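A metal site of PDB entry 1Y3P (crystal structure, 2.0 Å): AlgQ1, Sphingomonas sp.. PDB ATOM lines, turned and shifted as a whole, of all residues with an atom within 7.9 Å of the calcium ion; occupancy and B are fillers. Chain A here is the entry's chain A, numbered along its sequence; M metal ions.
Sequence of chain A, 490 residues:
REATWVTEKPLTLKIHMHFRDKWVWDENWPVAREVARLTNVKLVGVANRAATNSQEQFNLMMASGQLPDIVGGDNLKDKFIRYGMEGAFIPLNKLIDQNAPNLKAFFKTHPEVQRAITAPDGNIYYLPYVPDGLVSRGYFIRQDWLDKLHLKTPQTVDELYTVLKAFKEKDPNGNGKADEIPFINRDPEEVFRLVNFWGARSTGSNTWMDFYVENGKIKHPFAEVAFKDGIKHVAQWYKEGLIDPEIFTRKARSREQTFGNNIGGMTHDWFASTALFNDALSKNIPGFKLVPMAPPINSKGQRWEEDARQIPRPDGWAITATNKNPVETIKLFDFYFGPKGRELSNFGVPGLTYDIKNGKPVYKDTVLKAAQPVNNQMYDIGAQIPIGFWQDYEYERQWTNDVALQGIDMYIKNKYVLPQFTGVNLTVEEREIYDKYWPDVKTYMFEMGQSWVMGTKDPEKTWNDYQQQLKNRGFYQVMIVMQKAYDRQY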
ATOM      1  N   TRP A 145     -23.765  -2.415   9.970  1.00  0.00           N
ATOM      2  CA  TRP A 145     -24.618  -2.770  11.106  1.00  0.00           C
ATOM      3  C   TRP A 145     -25.084  -4.222  10.968  1.00  0.00           C
ATOM      4  O   TRP A 145     -25.160  -4.968  11.956  1.00  0.00           O
ATOM      5  CB  TRP A 145     -25.807  -1.821  11.196  1.00  0.00           C
ATOM      6  CG  TRP A 145     -25.480  -0.492  11.843  1.00  0.00           C
ATOM      7  CD1 TRP A 145     -24.242  -0.018  12.178  1.00  0.00           C
ATOM      8  CD2 TRP A 145     -26.416   0.516  12.261  1.00  0.00           C
ATOM      9  NE1 TRP A 145     -24.346   1.216  12.780  1.00  0.00           N
ATOM     10  CE2 TRP A 145     -25.672   1.564  12.846  1.00  0.00           C
ATOM     11  CE3 TRP A 145     -27.806   0.622  12.201  1.00  0.00           C
ATOM     12  CZ2 TRP A 145     -26.269   2.712  13.364  1.00  0.00           C
ATOM     13  CZ3 TRP A 145     -28.409   1.767  12.727  1.00  0.00           C
ATOM     14  CH2 TRP A 145     -27.641   2.796  13.296  1.00  0.00           C
ATOM     15  N   PHE A 167     -31.856  -3.355  14.744  1.00  0.00           N
ATOM     16  CA  PHE A 167     -31.173  -2.072  14.673  1.00  0.00           C
ATOM     17  C   PHE A 167     -31.591  -1.209  15.859  1.00  0.00           C
ATOM     18  O   PHE A 167     -30.785  -0.513  16.465  1.00  0.00           O
ATOM     19  CB  PHE A 167     -31.547  -1.330  13.382  1.00  0.00           C
ATOM     20  CG  PHE A 167     -30.827  -1.831  12.163  1.00  0.00           C
ATOM     21  CD1 PHE A 167     -29.898  -2.867  12.242  1.00  0.00           C
ATOM     22  CD2 PHE A 167     -31.048  -1.224  10.926  1.00  0.00           C
ATOM     23  CE1 PHE A 167     -29.194  -3.290  11.121  1.00  0.00           C
ATOM     24  CE2 PHE A 167     -30.355  -1.637   9.788  1.00  0.00           C
ATOM     25  CZ  PHE A 167     -29.429  -2.682   9.887  1.00  0.00           C
ATOM     26  N   LYS A 168     -32.884  -1.272  16.160  1.00  0.00           N
ATOM     27  CA  LYS A 168     -33.481  -0.502  17.235  1.00  0.00           C
ATOM     28  C   LYS A 168     -33.084  -0.969  18.626  1.00  0.00           C
ATOM     29  O   LYS A 168     -32.769  -0.148  19.488  1.00  0.00           O
ATOM     30  CB  LYS A 168     -35.008  -0.573  17.100  1.00  0.00           C
ATOM     31  CG  LYS A 168     -35.814   0.117  18.203  1.00  0.00           C
ATOM     32  CD  LYS A 168     -35.780   1.630  18.062  1.00  0.00           C
ATOM     33  CE  LYS A 168     -37.028   2.251  18.675  1.00  0.00           C
ATOM     34  NZ  LYS A 168     -37.212   1.849  20.094  1.00  0.00           N
ATOM     35  N   GLU A 169     -33.067  -2.280  18.843  1.00  0.00           N
ATOM     36  CA  GLU A 169     -32.797  -2.806  20.171  1.00  0.00           C
ATOM     37  C   GLU A 169     -31.439  -3.399  20.480  1.00  0.00           C
ATOM     38  O   GLU A 169     -31.090  -3.552  21.652  1.00  0.00           O
ATOM     39  CB  GLU A 169     -33.869  -3.852  20.512  1.00  0.00           C
ATOM     40  CG  GLU A 169     -35.293  -3.439  20.176  1.00  0.00           C
ATOM     41  CD  GLU A 169     -36.305  -4.546  20.419  1.00  0.00           C
ATOM     42  OE1 GLU A 169     -36.022  -5.705  20.074  1.00  0.00           O
ATOM     43  OE2 GLU A 169     -37.398  -4.250  20.948  1.00  0.00           O
ATOM     44  N   LYS A 170     -30.663  -3.737  19.456  1.00  0.00           N
ATOM     45  CA  LYS A 170     -29.362  -4.367  19.658  1.00  0.00           C
ATOM     46  C   LYS A 170     -28.131  -3.459  19.684  1.00  0.00           C
ATOM     47  O   LYS A 170     -27.009  -3.930  19.529  1.00  0.00           O
ATOM     48  CB  LYS A 170     -29.157  -5.476  18.625  1.00  0.00           C
ATOM     49  CG  LYS A 170     -30.250  -6.560  18.627  1.00  0.00           C
ATOM     50  CD  LYS A 170     -30.278  -7.374  19.930  1.00  0.00           C
ATOM     51  CE  LYS A 170     -30.973  -6.625  21.057  1.00  0.00           C
ATOM     52  NZ  LYS A 170     -31.017  -7.415  22.319  1.00  0.00           N
ATOM     53  N   ASP A 171     -28.358  -2.162  19.853  1.00  0.00           N
ATOM     54  CA  ASP A 171     -27.250  -1.217  19.960  1.00  0.00           C
ATOM     55  C   ASP A 171     -26.143  -1.426  18.923  1.00  0.00           C
ATOM     56  O   ASP A 171     -24.997  -1.676  19.282  1.00  0.00           O
ATOM     57  CB  ASP A 171     -26.662  -1.334  21.377  1.00  0.00           C
ATOM     58  CG  ASP A 171     -25.654  -0.252  21.673  1.00  0.00           C
ATOM     59  OD1 ASP A 171     -24.721  -0.503  22.459  1.00  0.00           O
ATOM     60  OD2 ASP A 171     -25.810   0.868  21.143  1.00  0.00           O
ATOM     61  N   PRO A 172     -26.474  -1.326  17.627  1.00  0.00           N
ATOM     62  CA  PRO A 172     -25.426  -1.526  16.617  1.00  0.00           C
ATOM     63  C   PRO A 172     -24.250  -0.543  16.671  1.00  0.00           C
ATOM     64  O   PRO A 172     -23.122  -0.945  16.380  1.00  0.00           O
ATOM     65  CB  PRO A 172     -26.196  -1.461  15.295  1.00  0.00           C
ATOM     66  CG  PRO A 172     -27.367  -0.577  15.616  1.00  0.00           C
ATOM     67  CD  PRO A 172     -27.785  -1.063  16.992  1.00  0.00           C
ATOM     68  N   ASN A 173     -24.474   0.727  17.024  1.00  0.00           N
ATOM     69  CA  ASN A 173     -23.338   1.648  17.078  1.00  0.00           C
ATOM     70  C   ASN A 173     -22.544   1.459  18.367  1.00  0.00           C
ATOM     71  O   ASN A 173     -21.575   2.175  18.634  1.00  0.00           O
ATOM     72  CB  ASN A 173     -23.765   3.131  16.910  1.00  0.00           C
ATOM     73  CG  ASN A 173     -24.708   3.627  17.995  1.00  0.00           C
ATOM     74  OD1 ASN A 173     -24.735   3.105  19.105  1.00  0.00           O
ATOM     75  ND2 ASN A 173     -25.467   4.670  17.667  1.00  0.00           N
ATOM     76  N   GLY A 174     -22.974   0.470  19.153  1.00  0.00           N
ATOM     77  CA  GLY A 174     -22.292   0.102  20.385  1.00  0.00           C
ATOM     78  C   GLY A 174     -21.965   1.119  21.460  1.00  0.00           C
ATOM     79  O   GLY A 174     -20.970   0.959  22.159  1.00  0.00           O
ATOM     80  N   ASN A 175     -22.802   2.136  21.630  1.00  0.00           N
ATOM     81  CA  ASN A 175     -22.533   3.130  22.657  1.00  0.00           C
ATOM     82  C   ASN A 175     -23.370   2.902  23.918  1.00  0.00           C
ATOM     83  O   ASN A 175     -23.444   3.763  24.792  1.00  0.00           O
ATOM     84  CB  ASN A 175     -22.767   4.546  22.111  1.00  0.00           C
ATOM     85  CG  ASN A 175     -24.186   4.780  21.658  1.00  0.00           C
ATOM     86  OD1 ASN A 175     -24.473   5.792  21.007  1.00  0.00           O
ATOM     87  ND2 ASN A 175     -25.097   3.876  21.999  1.00  0.00           N
ATOM     88  N   GLY A 176     -23.999   1.729  23.979  1.00  0.00           N
ATOM     89  CA  GLY A 176     -24.816   1.377  25.142  1.00  0.00           C
ATOM     90  C   GLY A 176     -26.112   2.141  25.276  1.00  0.00           C
ATOM     91  O   GLY A 176     -26.805   2.041  26.303  1.00  0.00           O
ATOM     92  N   LYS A 177     -26.453   2.921  24.253  1.00  0.00           N
ATOM     93  CA  LYS A 177     -27.683   3.697  24.272  1.00  0.00           C
ATOM     94  C   LYS A 177     -28.622   3.292  23.148  1.00  0.00           C
ATOM     95  O   LYS A 177     -28.184   2.894  22.068  1.00  0.00           O
ATOM     96  CB  LYS A 177     -27.352   5.193  24.128  1.00  0.00           C
ATOM     97  CG  LYS A 177     -26.543   5.753  25.285  1.00  0.00           C
ATOM     98  CD  LYS A 177     -26.205   7.229  25.087  1.00  0.00           C
ATOM     99  CE  LYS A 177     -25.231   7.433  23.939  1.00  0.00           C
ATOM    100  NZ  LYS A 177     -24.854   8.865  23.815  1.00  0.00           N
ATOM    101  N   ALA A 178     -29.922   3.369  23.422  1.00  0.00           N
ATOM    102  CA  ALA A 178     -30.942   3.023  22.432  1.00  0.00           C
ATOM    103  C   ALA A 178     -31.234   4.307  21.653  1.00  0.00           C
ATOM    104  O   ALA A 178     -32.288   4.919  21.821  1.00  0.00           O
ATOM    105  CB  ALA A 178     -32.202   2.529  23.138  1.00  0.00           C
ATOM    106  N   ASP A 179     -30.279   4.712  20.826  1.00  0.00           N
ATOM    107  CA  ASP A 179     -30.390   5.940  20.049  1.00  0.00           C
ATOM    108  C   ASP A 179     -30.619   5.689  18.560  1.00  0.00           C
ATOM    109  O   ASP A 179     -30.900   6.617  17.803  1.00  0.00           O
ATOM    110  CB  ASP A 179     -29.124   6.801  20.221  1.00  0.00           C
ATOM    111  CG  ASP A 179     -27.838   6.043  19.903  1.00  0.00           C
ATOM    112  OD1 ASP A 179     -26.780   6.693  19.782  1.00  0.00           O
ATOM    113  OD2 ASP A 179     -27.860   4.789  19.781  1.00  0.00           O
ATOM    114  N   GLU A 180     -30.500   4.428  18.137  1.00  0.00           N
ATOM    115  CA  GLU A 180     -30.682   4.079  16.732  1.00  0.00           C
ATOM    116  C   GLU A 180     -32.098   4.291  16.208  1.00  0.00           C
ATOM    117  O   GLU A 180     -33.077   3.997  16.895  1.00  0.00           O
ATOM    118  CB  GLU A 180     -30.285   2.619  16.490  1.00  0.00           C
ATOM    119  CG  GLU A 180     -28.802   2.330  16.544  1.00  0.00           C
ATOM    120  CD  GLU A 180     -28.255   2.144  17.956  1.00  0.00           C
ATOM    121  OE1 GLU A 180     -27.046   1.867  18.079  1.00  0.00           O
ATOM    122  OE2 GLU A 180     -29.039   2.270  18.931  1.00  0.00           O
ATOM    123  N   ASN A 262     -24.327   8.592  13.308  1.00  0.00           N
ATOM    124  CA  ASN A 262     -24.351   7.134  13.361  1.00  0.00           C
ATOM    125  C   ASN A 262     -25.573   6.532  14.065  1.00  0.00           C
ATOM    126  O   ASN A 262     -25.429   5.617  14.885  1.00  0.00           O
ATOM    127  CB  ASN A 262     -23.048   6.626  14.011  1.00  0.00           C
ATOM    128  CG  ASN A 262     -22.735   5.179  13.663  1.00  0.00           C
ATOM    129  OD1 ASN A 262     -23.359   4.594  12.780  1.00  0.00           O
ATOM    130  ND2 ASN A 262     -21.737   4.612  14.333  1.00  0.00           N
ATOM    131  N   ILE A 263     -26.763   7.031  13.747  1.00  0.00           N
ATOM    132  CA  ILE A 263     -27.998   6.495  14.326  1.00  0.00           C
ATOM    133  C   ILE A 263     -29.049   6.117  13.276  1.00  0.00           C
ATOM    134  O   ILE A 263     -30.125   5.631  13.615  1.00  0.00           O
ATOM    135  CB  ILE A 263     -28.636   7.469  15.351  1.00  0.00           C
ATOM    136  CG1 ILE A 263     -28.998   8.786  14.664  1.00  0.00           C
ATOM    137  CG2 ILE A 263     -27.661   7.693  16.506  1.00  0.00           C
ATOM    138  CD1 ILE A 263     -29.780   9.733  15.525  1.00  0.00           C
HETATM  139 CA    CA M   1     -26.675   2.727  20.394  1.00  0.00          CA
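The calcium ion is bound by OD2 of Asp 171 (2.2 Å). O of Lys 177 binds the calcium ion (2.3 Å). The calcium ion is bound by the side-chain amide oxygen (OD1) of Asn 173, 2.4 Å away. The side-chain carboxylate (OD2) of Asp 179 binds the calcium ion (2.5 Å). OE1 of Glu 180 is bound to the calcium ion. ND2 of Asn 175 is bound to the calcium ion (2.5 Å). OE2 of Glu 180 binds the calcium ion.
Six residues have an atom within 4 Å of the calcium ion: Asp 171, Asn 173, Asn 175, Lys 177, Asp 179 and Glu 180.
The side-chain carboxylate (OD2) of Asp 171 sits close to the backbone NH (N) of Gly 174, at 3.5 Å. The side-chain amide nitrogen of Asn 173 lies within hydrogen-bond range of the backbone carbonyl oxygen of Asn 262. OD1 of Asp 171 lies within hydrogen-bond range of N of Gly 176 (2.8 Å).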
